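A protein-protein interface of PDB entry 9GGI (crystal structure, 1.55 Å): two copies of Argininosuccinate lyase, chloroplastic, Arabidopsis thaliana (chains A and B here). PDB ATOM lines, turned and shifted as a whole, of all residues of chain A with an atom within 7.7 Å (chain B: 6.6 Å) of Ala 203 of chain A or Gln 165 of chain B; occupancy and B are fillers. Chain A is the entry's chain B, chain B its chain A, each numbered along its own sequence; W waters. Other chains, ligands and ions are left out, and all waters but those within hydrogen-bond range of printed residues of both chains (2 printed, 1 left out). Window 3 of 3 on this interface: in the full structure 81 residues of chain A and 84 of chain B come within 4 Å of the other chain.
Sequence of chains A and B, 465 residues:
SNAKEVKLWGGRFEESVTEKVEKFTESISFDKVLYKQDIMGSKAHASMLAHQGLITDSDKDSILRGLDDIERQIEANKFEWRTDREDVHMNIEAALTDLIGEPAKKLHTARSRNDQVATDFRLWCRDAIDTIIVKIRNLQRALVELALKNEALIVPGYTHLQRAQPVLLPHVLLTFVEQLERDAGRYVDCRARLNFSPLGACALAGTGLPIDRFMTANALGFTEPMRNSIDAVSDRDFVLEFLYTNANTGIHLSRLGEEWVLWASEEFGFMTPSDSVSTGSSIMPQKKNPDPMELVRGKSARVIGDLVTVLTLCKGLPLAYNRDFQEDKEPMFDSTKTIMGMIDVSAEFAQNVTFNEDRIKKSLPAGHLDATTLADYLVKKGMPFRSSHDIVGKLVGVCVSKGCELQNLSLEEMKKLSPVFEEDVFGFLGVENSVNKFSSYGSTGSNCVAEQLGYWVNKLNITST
Among the printed residues, pairs that only touch across the chains: Asn 114 of chain A with Thr 159 of chain B (3.8 Å), Ala 203 of chain A with Thr 159 of chain B (3.7 Å), Ala 203 of chain A with Gln 165 of chain B (3.8 Å), Leu 204 of chain A with Gly 157 of chain B (3.7 Å), Leu 204 of chain A with Tyr 158 of chain B (3.6 Å), Leu 204 of chain A with Ala 164 of chain B (3.9 Å), Leu 204 of chain A with Gln 165 of chain B (3.1 Å), Ala 205 of chain A with Gln 165 of chain B (3.5 Å), Ala 205 of chain A with Val 167 of chain B (3.9 Å), Ala 205 of chain A with Phe 438 of chain B (3.4 Å), Gly 206 of chain A with Gln 165 of chain B (3.7 Å), Gly 206 of chain A with Phe 438 of chain B (3.4 Å), Thr 207 of chain A with Asp 376 of chain B (3.6 Å), Thr 207 of chain A with Phe 438 of chain B (3.7 Å) and Tyr 321 of chain A with Thr 159 of chain B (3.3 Å).
Printed residues of chain A that touch a printed residue of chain B: Asn 114, Ala 203, Leu 204, Ala 205, Gly 206, Thr 207, Gly 208, Ala 320 and Tyr 321.
Of the 18 printed residues of chain B, 9 touch a printed residue of chain A.
Hydrophobic or aromatic side chains of chain B that line the printed part of chain A: Ala 164, Val 167 and Phe 438.
The backbone carbonyl oxygen (O) of Val 167 of chain B lies within hydrogen-bond range of the backbone NH (N) of Val 155 of chain B (2.9 Å).
The backbone carbonyl oxygen (O) of Gly 157 of chain B sits at hydrogen-bond distance from the backbone NH (N) of Ala 164 of chain B (2.8 Å).
The backbone carbonyl oxygen of Ala 203 of chain A lies within hydrogen-bond range of the side-chain amide nitrogen of Asn 114 of chain A, at 3.0 Å.
The backbone carbonyl oxygen (O) of Ala 201 of chain A lies within hydrogen-bond range of the backbone NH (N) of Gly 206 of chain A.
Water W2 lies within hydrogen-bond range of OD1 of Asp 376 of chain B (2.7 Å) and OG1 of Thr 207 of chain A (2.7 Å).
Water W1 bridges the backbone carbonyl oxygen of Gly 206 of chain A (2.8 Å) and the side-chain amide oxygen of Gln 165 of chain B (2.9 Å).
Printed residues of chain B within 4 Å of Ala 203 of chain A: Thr 159 and Gln 165.
Printed residues of chain A within 4 Å of Gln 165 of chain B: Ala 203, Leu 204, Ala 205 and Gly 206.
No residue of chain A comes within 4 Å of Pro 166 of chain B.
Of the printed residues of chain B, Tyr 321 of chain A touches Thr 159.
Of the printed residues of chain A, Tyr 158 of chain B touches Leu 204 (3.6 Å) and Ala 320 (2.9 Å).
Of the printed residues of chain A, Asp 376 of chain B touches Thr 207 and Gly 208.
Of the printed residues of chain B, Leu 204 of chain A touches Gly 157, Tyr 158, Ala 164 and Gln 165.
Thr 373 of chain B touches none of the printed residues of chain A.
Ala 232 of chain A touches none of the printed residues of chain B.
The nearest printed residue of chain A that does not touch Gln 165 of chain B is Cys 202 of chain A (5.5 Å).
The nearest printed residue of chain B that does not touch Gly 208 of chain A is Phe 438 of chain B (4.2 Å).
The backbone carbonyl oxygen (O) of Tyr 158 of chain B is in hydrogen-bond range of the backbone NH (N) of Ala 320 of chain A (2.9 Å).
The backbone NH of Gly 208 of chain A lies within hydrogen-bond range of the side-chain carboxylate of Asp 376 of chain B (3.1 Å).
O of Ala 205 of chain A sits at hydrogen-bond distance from N of Thr 444 of chain B (3.1 Å).
No position is printed for both chains.
Of the 18 pairs that touch across the chains among the printed residues, none has its exchanged pair printed and touching as well.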
ATOM      1  N   ALA A 110      -5.573 -30.032   0.168  1.00  0.00           N
ATOM      2  CA  ALA A 110      -5.408 -31.103   1.128  1.00  0.00           C
ATOM      3  C   ALA A 110      -3.984 -31.612   1.099  1.00  0.00           C
ATOM      4  O   ALA A 110      -3.774 -32.793   1.259  1.00  0.00           O
ATOM      5  CB  ALA A 110      -6.366 -32.263   0.878  1.00  0.00           C
ATOM      6  N   ARG A 111      -3.021 -30.706   1.024  1.00  0.00           N
ATOM      7  CA  ARG A 111      -1.606 -31.047   1.106  1.00  0.00           C
ATOM      8  C   ARG A 111      -0.850 -29.836   1.646  1.00  0.00           C
ATOM      9  O   ARG A 111      -1.242 -28.681   1.455  1.00  0.00           O
ATOM     10  CB  ARG A 111      -1.084 -31.371  -0.313  1.00  0.00           C
ATOM     11  CG  ARG A 111       0.304 -32.018  -0.320  1.00  0.00           C
ATOM     12  CD  ARG A 111       0.760 -32.486  -1.695  1.00  0.00           C
ATOM     13  NE  ARG A 111       0.967 -31.306  -2.522  1.00  0.00           N
ATOM     14  CZ  ARG A 111       1.459 -31.274  -3.755  1.00  0.00           C
ATOM     15  NH1 ARG A 111       1.897 -32.357  -4.299  1.00  0.00           N
ATOM     16  NH2 ARG A 111       1.631 -30.103  -4.319  1.00  0.00           N
ATOM     17  N   SER A 112       0.269 -30.099   2.319  1.00  0.00           N
ATOM     18  CA  SER A 112       1.211 -29.100   2.794  1.00  0.00           C
ATOM     19  C   SER A 112       2.574 -29.360   2.186  1.00  0.00           C
ATOM     20  O   SER A 112       2.913 -30.471   1.766  1.00  0.00           O
ATOM     21  CB  SER A 112       1.274 -29.203   4.320  1.00  0.00           C
ATOM     22  OG  SER A 112       2.306 -28.388   4.867  1.00  0.00           O
ATOM     23  N   ARG A 113       3.435 -28.343   2.167  1.00  0.00           N
ATOM     24  CA  ARG A 113       4.824 -28.609   1.865  1.00  0.00           C
ATOM     25  C   ARG A 113       5.388 -29.587   2.890  1.00  0.00           C
ATOM     26  O   ARG A 113       6.373 -30.254   2.608  1.00  0.00           O
ATOM     27  CB  ARG A 113       5.656 -27.336   1.835  1.00  0.00           C
ATOM     28  CG  ARG A 113       5.321 -26.468   0.620  1.00  0.00           C
ATOM     29  CD  ARG A 113       5.600 -27.136  -0.745  1.00  0.00           C
ATOM     30  NE  ARG A 113       5.560 -26.142  -1.825  1.00  0.00           N
ATOM     31  CZ  ARG A 113       4.642 -26.189  -2.830  1.00  0.00           C
ATOM     32  NH1 ARG A 113       3.907 -27.289  -3.030  1.00  0.00           N
ATOM     33  NH2 ARG A 113       4.512 -25.122  -3.645  1.00  0.00           N
ATOM     34  N   ASN A 114       4.841 -29.580   4.111  1.00  0.00           N
ATOM     35  CA  ASN A 114       5.448 -30.381   5.186  1.00  0.00           C
ATOM     36  C   ASN A 114       5.327 -31.888   4.915  1.00  0.00           C
ATOM     37  O   ASN A 114       6.282 -32.626   5.138  1.00  0.00           O
ATOM     38  CB  ASN A 114       4.800 -30.069   6.540  1.00  0.00           C
ATOM     39  CG  ASN A 114       4.969 -28.632   6.987  1.00  0.00           C
ATOM     40  OD1 ASN A 114       5.707 -27.879   6.345  1.00  0.00           O
ATOM     41  ND2 ASN A 114       4.251 -28.216   8.026  1.00  0.00           N
ATOM     42  N   ASP A 115       4.157 -32.369   4.464  1.00  0.00           N
ATOM     43  CA  ASP A 115       3.981 -33.774   4.121  1.00  0.00           C
ATOM     44  C   ASP A 115       4.543 -34.062   2.723  1.00  0.00           C
ATOM     45  O   ASP A 115       5.051 -35.146   2.465  1.00  0.00           O
ATOM     46  CB  ASP A 115       2.573 -34.275   4.396  1.00  0.00           C
ATOM     47  CG  ASP A 115       1.456 -33.695   3.553  1.00  0.00           C
ATOM     48  OD1 ASP A 115       1.537 -32.503   3.254  1.00  0.00           O
ATOM     49  OD2 ASP A 115       0.457 -34.386   3.349  1.00  0.00           O
ATOM     50  N   GLY A 200      -0.534 -36.976   3.246  1.00  0.00           N
ATOM     51  CA  GLY A 200      -1.869 -36.843   3.804  1.00  0.00           C
ATOM     52  C   GLY A 200      -1.864 -36.467   5.274  1.00  0.00           C
ATOM     53  O   GLY A 200      -2.916 -36.314   5.863  1.00  0.00           O
ATOM     54  N   ALA A 201      -0.653 -36.327   5.850  1.00  0.00           N
ATOM     55  CA  ALA A 201      -0.553 -35.679   7.149  1.00  0.00           C
ATOM     56  C   ALA A 201      -0.828 -34.196   7.106  1.00  0.00           C
ATOM     57  O   ALA A 201      -1.058 -33.595   8.149  1.00  0.00           O
ATOM     58  CB  ALA A 201       0.829 -35.952   7.706  1.00  0.00           C
ATOM     59  N   CYS A 202      -0.735 -33.591   5.916  1.00  0.00           N
ATOM     60  CA  CYS A 202      -0.914 -32.144   5.767  1.00  0.00           C
ATOM     61  C   CYS A 202       0.085 -31.405   6.640  1.00  0.00           C
ATOM     62  O   CYS A 202       1.247 -31.823   6.689  1.00  0.00           O
ATOM     63  CB  CYS A 202      -2.387 -31.773   5.910  1.00  0.00           C
ATOM     64  SG  CYS A 202      -3.419 -32.487   4.608  1.00  0.00           S
ATOM     65  N   ALA A 203      -0.276 -30.250   7.243  1.00  0.00           N
ATOM     66  CA  ALA A 203       0.712 -29.480   7.982  1.00  0.00           C
ATOM     67  C   ALA A 203       1.292 -30.240   9.177  1.00  0.00           C
ATOM     68  O   ALA A 203       2.446 -30.024   9.513  1.00  0.00           O
ATOM     69  CB  ALA A 203       0.153 -28.142   8.424  1.00  0.00           C
ATOM     70  N   LEU A 204       0.422 -30.995   9.853  1.00  0.00           N
ATOM     71  CA  LEU A 204       0.792 -31.835  10.981  1.00  0.00           C
ATOM     72  C   LEU A 204      -0.376 -32.621  11.575  1.00  0.00           C
ATOM     73  O   LEU A 204      -0.102 -33.644  12.199  1.00  0.00           O
ATOM     74  CB  LEU A 204       1.449 -31.073  12.128  1.00  0.00           C
ATOM     75  CG  LEU A 204       0.524 -30.347  13.106  1.00  0.00           C
ATOM     76  CD1 LEU A 204       1.317 -29.952  14.338  1.00  0.00           C
ATOM     77  CD2 LEU A 204      -0.065 -29.132  12.445  1.00  0.00           C
ATOM     78  N   ALA A 205      -1.622 -32.229  11.334  1.00  0.00           N
ATOM     79  CA  ALA A 205      -2.757 -32.780  12.061  1.00  0.00           C
ATOM     80  C   ALA A 205      -3.698 -33.601  11.203  1.00  0.00           C
ATOM     81  O   ALA A 205      -4.711 -34.097  11.705  1.00  0.00           O
ATOM     82  CB  ALA A 205      -3.529 -31.642  12.710  1.00  0.00           C
ATOM     83  N   GLY A 206      -3.374 -33.733   9.908  1.00  0.00           N
ATOM     84  CA  GLY A 206      -4.299 -34.295   8.941  1.00  0.00           C
ATOM     85  C   GLY A 206      -5.260 -33.255   8.369  1.00  0.00           C
ATOM     86  O   GLY A 206      -4.977 -32.050   8.379  1.00  0.00           O
ATOM     87  N   THR A 207      -6.401 -33.757   7.891  1.00  0.00           N
ATOM     88  CA  THR A 207      -7.365 -32.908   7.202  1.00  0.00           C
ATOM     89  C   THR A 207      -8.760 -33.425   7.478  1.00  0.00           C
ATOM     90  O   THR A 207      -8.931 -34.580   7.811  1.00  0.00           O
ATOM     91  CB  THR A 207      -7.031 -32.848   5.719  1.00  0.00           C
ATOM     92  OG1 THR A 207      -8.006 -31.996   5.078  1.00  0.00           O
ATOM     93  CG2 THR A 207      -7.073 -34.190   5.043  1.00  0.00           C
ATOM     94  N   GLY A 208      -9.756 -32.554   7.271  1.00  0.00           N
ATOM     95  CA  GLY A 208     -11.157 -32.943   7.201  1.00  0.00           C
ATOM     96  C   GLY A 208     -11.638 -33.161   5.780  1.00  0.00           C
ATOM     97  O   GLY A 208     -12.787 -33.550   5.598  1.00  0.00           O
ATOM     98  N   SER A 229       0.016 -38.373  12.005  1.00  0.00           N
ATOM     99  CA  SER A 229       0.277 -37.173  11.170  1.00  0.00           C
ATOM    100  C   SER A 229       1.436 -36.316  11.722  1.00  0.00           C
ATOM    101  O   SER A 229       2.205 -35.807  10.935  1.00  0.00           O
ATOM    102  CB  SER A 229      -1.013 -36.363  11.054  1.00  0.00           C
ATOM    103  OG  SER A 229      -1.452 -35.872  12.304  1.00  0.00           O
ATOM    104  N   ILE A 230       1.497 -36.183  13.052  1.00  0.00           N
ATOM    105  CA  ILE A 230       2.555 -35.361  13.599  1.00  0.00           C
ATOM    106  C   ILE A 230       3.898 -36.030  13.362  1.00  0.00           C
ATOM    107  O   ILE A 230       4.891 -35.380  12.989  1.00  0.00           O
ATOM    108  CB  ILE A 230       2.290 -35.052  15.069  1.00  0.00           C
ATOM    109  CG1 ILE A 230       0.935 -34.310  15.304  1.00  0.00           C
ATOM    110  CG2 ILE A 230       3.496 -34.343  15.692  1.00  0.00           C
ATOM    111  CD1 ILE A 230       0.549 -34.223  16.788  1.00  0.00           C
ATOM    112  N   ALA A 232       4.551 -38.063  10.969  1.00  0.00           N
ATOM    113  CA  ALA A 232       4.835 -38.049   9.549  1.00  0.00           C
ATOM    114  C   ALA A 232       5.589 -36.792   9.115  1.00  0.00           C
ATOM    115  O   ALA A 232       6.427 -36.827   8.239  1.00  0.00           O
ATOM    116  CB  ALA A 232       3.512 -38.125   8.822  1.00  0.00           C
ATOM    117  N   VAL A 233       5.229 -35.625   9.685  1.00  0.00           N
ATOM    118  CA  VAL A 233       5.871 -34.382   9.245  1.00  0.00           C
ATOM    119  C   VAL A 233       7.138 -34.083  10.062  1.00  0.00           C
ATOM    120  O   VAL A 233       7.936 -33.250   9.634  1.00  0.00           O
ATOM    121  CB  VAL A 233       4.928 -33.176   9.277  1.00  0.00           C
ATOM    122  CG1 VAL A 233       3.737 -33.377   8.368  1.00  0.00           C
ATOM    123  CG2 VAL A 233       4.493 -32.783  10.675  1.00  0.00           C
ATOM    124  N   SER A 234       7.337 -34.735  11.209  1.00  0.00           N
ATOM    125  CA  SER A 234       8.406 -34.423  12.149  1.00  0.00           C
ATOM    126  C   SER A 234       9.543 -35.426  12.090  1.00  0.00           C
ATOM    127  O   SER A 234      10.582 -35.194  12.675  1.00  0.00           O
ATOM    128  CB  SER A 234       7.900 -34.304  13.568  1.00  0.00           C
ATOM    129  OG  SER A 234       7.380 -35.536  14.002  1.00  0.00           O
ATOM    130  N   ALA A 320       6.486 -29.759  15.656  1.00  0.00           N
ATOM    131  CA  ALA A 320       6.457 -30.944  14.812  1.00  0.00           C
ATOM    132  C   ALA A 320       7.462 -30.749  13.664  1.00  0.00           C
ATOM    133  O   ALA A 320       8.649 -31.139  13.776  1.00  0.00           O
ATOM    134  CB  ALA A 320       5.063 -31.159  14.332  1.00  0.00           C
ATOM    135  N   TYR A 321       7.046 -29.989  12.638  1.00  0.00           N
ATOM    136  CA  TYR A 321       7.933 -29.531  11.573  1.00  0.00           C
ATOM    137  C   TYR A 321       8.618 -28.217  11.976  1.00  0.00           C
ATOM    138  O   TYR A 321       8.014 -27.283  12.490  1.00  0.00           O
ATOM    139  CB  TYR A 321       7.162 -29.337  10.255  1.00  0.00           C
ATOM    140  CG  TYR A 321       8.076 -28.809   9.153  1.00  0.00           C
ATOM    141  CD1 TYR A 321       8.930 -29.660   8.456  1.00  0.00           C
ATOM    142  CD2 TYR A 321       8.151 -27.440   8.876  1.00  0.00           C
ATOM    143  CE1 TYR A 321       9.811 -29.166   7.490  1.00  0.00           C
ATOM    144  CE2 TYR A 321       9.095 -26.933   7.996  1.00  0.00           C
ATOM    145  CZ  TYR A 321       9.904 -27.799   7.289  1.00  0.00           C
ATOM    146  OH  TYR A 321      10.847 -27.281   6.423  1.00  0.00           O
ATOM    147  N   VAL B 155      -4.549 -29.477  22.855  1.00  0.00           N
ATOM    148  CA  VAL B 155      -3.486 -28.493  22.936  1.00  0.00           C
ATOM    149  C   VAL B 155      -3.233 -27.938  21.536  1.00  0.00           C
ATOM    150  O   VAL B 155      -3.608 -28.549  20.544  1.00  0.00           O
ATOM    151  CB  VAL B 155      -2.211 -29.107  23.534  1.00  0.00           C
ATOM    152  CG1 VAL B 155      -2.425 -29.496  25.004  1.00  0.00           C
ATOM    153  CG2 VAL B 155      -1.740 -30.338  22.758  1.00  0.00           C
ATOM    154  N   PRO B 156      -2.505 -26.831  21.377  1.00  0.00           N
ATOM    155  CA  PRO B 156      -2.041 -26.389  20.059  1.00  0.00           C
ATOM    156  C   PRO B 156      -1.037 -27.404  19.508  1.00  0.00           C
ATOM    157  O   PRO B 156      -0.259 -27.994  20.276  1.00  0.00           O
ATOM    158  CB  PRO B 156      -1.450 -25.030  20.293  1.00  0.00           C
ATOM    159  CG  PRO B 156      -1.870 -24.645  21.646  1.00  0.00           C
ATOM    160  CD  PRO B 156      -1.988 -25.957  22.433  1.00  0.00           C
ATOM    161  N   GLY B 157      -1.078 -27.607  18.203  1.00  0.00           N
ATOM    162  CA  GLY B 157      -0.046 -28.280  17.444  1.00  0.00           C
ATOM    163  C   GLY B 157       0.800 -27.235  16.732  1.00  0.00           C
ATOM    164  O   GLY B 157       0.273 -26.251  16.221  1.00  0.00           O
ATOM    165  N   TYR B 158       2.119 -27.403  16.749  1.00  0.00           N
ATOM    166  CA  TYR B 158       3.013 -26.382  16.282  1.00  0.00           C
ATOM    167  C   TYR B 158       3.848 -26.781  15.075  1.00  0.00           C
ATOM    168  O   TYR B 158       4.294 -27.909  14.968  1.00  0.00           O
ATOM    169  CB  TYR B 158       4.029 -26.080  17.401  1.00  0.00           C
ATOM    170  CG  TYR B 158       3.384 -25.558  18.670  1.00  0.00           C
ATOM    171  CD1 TYR B 158       2.903 -26.461  19.619  1.00  0.00           C
ATOM    172  CD2 TYR B 158       3.234 -24.211  18.916  1.00  0.00           C
ATOM    173  CE1 TYR B 158       2.280 -26.000  20.771  1.00  0.00           C
ATOM    174  CE2 TYR B 158       2.615 -23.753  20.080  1.00  0.00           C
ATOM    175  CZ  TYR B 158       2.174 -24.661  21.014  1.00  0.00           C
ATOM    176  OH  TYR B 158       1.504 -24.255  22.151  1.00  0.00           O
ATOM    177  N   THR B 159       4.065 -25.795  14.209  1.00  0.00           N
ATOM    178  CA  THR B 159       5.127 -25.828  13.209  1.00  0.00           C
ATOM    179  C   THR B 159       5.880 -24.515  13.351  1.00  0.00           C
ATOM    180  O   THR B 159       5.292 -23.450  13.454  1.00  0.00           O
ATOM    181  CB  THR B 159       4.643 -26.090  11.787  1.00  0.00           C
ATOM    182  OG1 THR B 159       3.896 -24.986  11.337  1.00  0.00           O
ATOM    183  CG2 THR B 159       3.840 -27.370  11.747  1.00  0.00           C
ATOM    184  N   GLN B 162       5.111 -22.070  16.024  1.00  0.00           N
ATOM    185  CA  GLN B 162       3.943 -21.254  15.864  1.00  0.00           C
ATOM    186  C   GLN B 162       2.729 -22.173  15.849  1.00  0.00           C
ATOM    187  O   GLN B 162       2.734 -23.290  15.297  1.00  0.00           O
ATOM    188  CB  GLN B 162       3.997 -20.491  14.558  1.00  0.00           C
ATOM    189  CG  GLN B 162       5.117 -19.493  14.473  1.00  0.00           C
ATOM    190  CD  GLN B 162       4.854 -18.326  15.385  1.00  0.00           C
ATOM    191  OE1 GLN B 162       3.759 -17.738  15.335  1.00  0.00           O
ATOM    192  NE2 GLN B 162       5.838 -17.917  16.164  1.00  0.00           N
ATOM    193  N   ARG B 163       1.646 -21.659  16.414  1.00  0.00           N
ATOM    194  CA  ARG B 163       0.395 -22.417  16.479  1.00  0.00           C
ATOM    195  C   ARG B 163      -0.174 -22.663  15.101  1.00  0.00           C
ATOM    196  O   ARG B 163      -0.360 -21.744  14.314  1.00  0.00           O
ATOM    197  CB  ARG B 163      -0.605 -21.619  17.325  1.00  0.00           C
ATOM    198  CG  ARG B 163      -0.209 -21.572  18.774  1.00  0.00           C
ATOM    199  CD  ARG B 163      -1.304 -20.810  19.511  1.00  0.00           C
ATOM    200  NE  ARG B 163      -1.022 -20.940  20.922  1.00  0.00           N
ATOM    201  CZ  ARG B 163      -1.931 -20.973  21.881  1.00  0.00           C
ATOM    202  NH1 ARG B 163      -3.226 -20.841  21.559  1.00  0.00           N
ATOM    203  NH2 ARG B 163      -1.522 -21.171  23.111  1.00  0.00           N
ATOM    204  N   ALA B 164      -0.419 -23.934  14.765  1.00  0.00           N
ATOM    205  CA  ALA B 164      -0.817 -24.286  13.400  1.00  0.00           C
ATOM    206  C   ALA B 164      -2.244 -24.831  13.382  1.00  0.00           C
ATOM    207  O   ALA B 164      -3.109 -24.300  12.660  1.00  0.00           O
ATOM    208  CB  ALA B 164       0.179 -25.284  12.820  1.00  0.00           C
ATOM    209  N   GLN B 165      -2.436 -25.939  14.052  1.00  0.00           N
ATOM    210  CA  GLN B 165      -3.793 -26.543  14.175  1.00  0.00           C
ATOM    211  C   GLN B 165      -3.986 -27.138  15.614  1.00  0.00           C
ATOM    212  O   GLN B 165      -3.056 -27.398  16.489  1.00  0.00           O
ATOM    213  CB  GLN B 165      -3.890 -27.695  13.184  1.00  0.00           C
ATOM    214  CG  GLN B 165      -4.264 -27.271  11.769  1.00  0.00           C
ATOM    215  CD  GLN B 165      -3.906 -28.319  10.743  1.00  0.00           C
ATOM    216  OE1 GLN B 165      -4.710 -28.710   9.893  1.00  0.00           O
ATOM    217  NE2 GLN B 165      -2.687 -28.817  10.838  1.00  0.00           N
ATOM    218  N   PRO B 166      -5.233 -27.365  16.009  1.00  0.00           N
ATOM    219  CA  PRO B 166      -5.466 -27.948  17.329  1.00  0.00           C
ATOM    220  C   PRO B 166      -5.298 -29.449  17.233  1.00  0.00           C
ATOM    221  O   PRO B 166      -5.660 -30.062  16.200  1.00  0.00           O
ATOM    222  CB  PRO B 166      -6.864 -27.513  17.645  1.00  0.00           C
ATOM    223  CG  PRO B 166      -7.549 -27.509  16.292  1.00  0.00           C
ATOM    224  CD  PRO B 166      -6.492 -27.161  15.263  1.00  0.00           C
ATOM    225  N   VAL B 167      -4.703 -30.046  18.288  1.00  0.00           N
ATOM    226  CA  VAL B 167      -4.490 -31.480  18.294  1.00  0.00           C
ATOM    227  C   VAL B 167      -4.896 -32.041  19.655  1.00  0.00           C
ATOM    228  O   VAL B 167      -4.850 -31.351  20.682  1.00  0.00           O
ATOM    229  CB  VAL B 167      -3.037 -31.874  17.989  1.00  0.00           C
ATOM    230  CG1 VAL B 167      -2.704 -31.433  16.543  1.00  0.00           C
ATOM    231  CG2 VAL B 167      -2.063 -31.258  18.973  1.00  0.00           C
ATOM    232  N   LEU B 369      -6.985 -21.401  15.699  1.00  0.00           N
ATOM    233  CA  LEU B 369      -6.604 -22.763  15.359  1.00  0.00           C
ATOM    234  C   LEU B 369      -7.660 -23.443  14.494  1.00  0.00           C
ATOM    235  O   LEU B 369      -7.384 -24.456  13.858  1.00  0.00           O
ATOM    236  CB  LEU B 369      -6.391 -23.490  16.675  1.00  0.00           C
ATOM    237  CG  LEU B 369      -5.171 -23.102  17.523  1.00  0.00           C
ATOM    238  CD1 LEU B 369      -5.130 -23.844  18.830  1.00  0.00           C
ATOM    239  CD2 LEU B 369      -3.955 -23.513  16.762  1.00  0.00           C
ATOM    240  N   ASP B 370      -8.858 -22.852  14.447  1.00  0.00           N
ATOM    241  CA  ASP B 370      -9.948 -23.386  13.651  1.00  0.00           C
ATOM    242  C   ASP B 370      -9.891 -22.944  12.205  1.00  0.00           C
ATOM    243  O   ASP B 370     -10.773 -23.285  11.402  1.00  0.00           O
ATOM    244  CB  ASP B 370     -11.287 -23.060  14.298  1.00  0.00           C
ATOM    245  CG  ASP B 370     -11.534 -21.639  14.757  1.00  0.00           C
ATOM    246  OD1 ASP B 370     -10.595 -20.798  14.699  1.00  0.00           O
ATOM    247  OD2 ASP B 370     -12.713 -21.357  15.077  1.00  0.00           O
ATOM    248  N   THR B 372      -8.154 -23.671   9.531  1.00  0.00           N
ATOM    249  CA  THR B 372      -8.066 -24.664   8.474  1.00  0.00           C
ATOM    250  C   THR B 372      -9.401 -25.418   8.353  1.00  0.00           C
ATOM    251  O   THR B 372      -9.751 -25.851   7.269  1.00  0.00           O
ATOM    252  CB  THR B 372      -6.876 -25.582   8.742  1.00  0.00           C
ATOM    253  OG1 THR B 372      -5.734 -24.719   8.813  1.00  0.00           O
ATOM    254  CG2 THR B 372      -6.647 -26.599   7.647  1.00  0.00           C
ATOM    255  N   THR B 373     -10.089 -25.657   9.486  1.00  0.00           N
ATOM    256  CA  THR B 373     -11.393 -26.319   9.445  1.00  0.00           C
ATOM    257  C   THR B 373     -12.384 -25.454   8.676  1.00  0.00           C
ATOM    258  O   THR B 373     -13.193 -25.957   7.899  1.00  0.00           O
ATOM    259  CB  THR B 373     -11.852 -26.575  10.891  1.00  0.00           C
ATOM    260  OG1 THR B 373     -10.845 -27.341  11.561  1.00  0.00           O
ATOM    261  CG2 THR B 373     -13.164 -27.334  10.970  1.00  0.00           C
ATOM    262  N   ASP B 376     -11.699 -25.841   5.115  1.00  0.00           N
ATOM    263  CA  ASP B 376     -12.174 -27.158   4.665  1.00  0.00           C
ATOM    264  C   ASP B 376     -13.683 -27.112   4.473  1.00  0.00           C
ATOM    265  O   ASP B 376     -14.207 -27.616   3.471  1.00  0.00           O
ATOM    266  CB  ASP B 376     -11.853 -28.281   5.617  1.00  0.00           C
ATOM    267  CG  ASP B 376     -10.382 -28.694   5.747  1.00  0.00           C
ATOM    268  OD1 ASP B 376      -9.570 -28.157   4.935  1.00  0.00           O
ATOM    269  OD2 ASP B 376     -10.085 -29.482   6.668  1.00  0.00           O
ATOM    270  N   PHE B 438     -11.457 -33.275  11.883  1.00  0.00           N
ATOM    271  CA  PHE B 438     -10.378 -34.010  11.235  1.00  0.00           C
ATOM    272  C   PHE B 438     -10.816 -35.464  11.056  1.00  0.00           C
ATOM    273  O   PHE B 438     -11.423 -36.064  11.957  1.00  0.00           O
ATOM    274  CB  PHE B 438      -9.099 -33.948  12.085  1.00  0.00           C
ATOM    275  CG  PHE B 438      -8.425 -32.618  12.065  1.00  0.00           C
ATOM    276  CD1 PHE B 438      -7.535 -32.279  11.055  1.00  0.00           C
ATOM    277  CD2 PHE B 438      -8.620 -31.709  13.095  1.00  0.00           C
ATOM    278  CE1 PHE B 438      -6.880 -31.062  11.028  1.00  0.00           C
ATOM    279  CE2 PHE B 438      -7.947 -30.483  13.079  1.00  0.00           C
ATOM    280  CZ  PHE B 438      -7.110 -30.135  12.022  1.00  0.00           C
ATOM    281  N   THR B 444      -5.595 -36.081  13.850  1.00  0.00           N
ATOM    282  CA  THR B 444      -5.996 -35.843  15.242  1.00  0.00           C
ATOM    283  C   THR B 444      -7.501 -35.956  15.486  1.00  0.00           C
ATOM    284  O   THR B 444      -7.924 -35.682  16.627  1.00  0.00           O
ATOM    285  CB  THR B 444      -5.558 -34.429  15.676  1.00  0.00           C
ATOM    286  OG1 THR B 444      -5.718 -34.436  17.106  1.00  0.00           O
ATOM    287  CG2 THR B 444      -6.286 -33.314  15.004  1.00  0.00           C
HETATM  288  O   HOH W   1      -5.471 -29.592   7.231  1.00  0.00           O
HETATM  289  O   HOH W   2      -7.191 -29.376   4.980  1.00  0.00           O
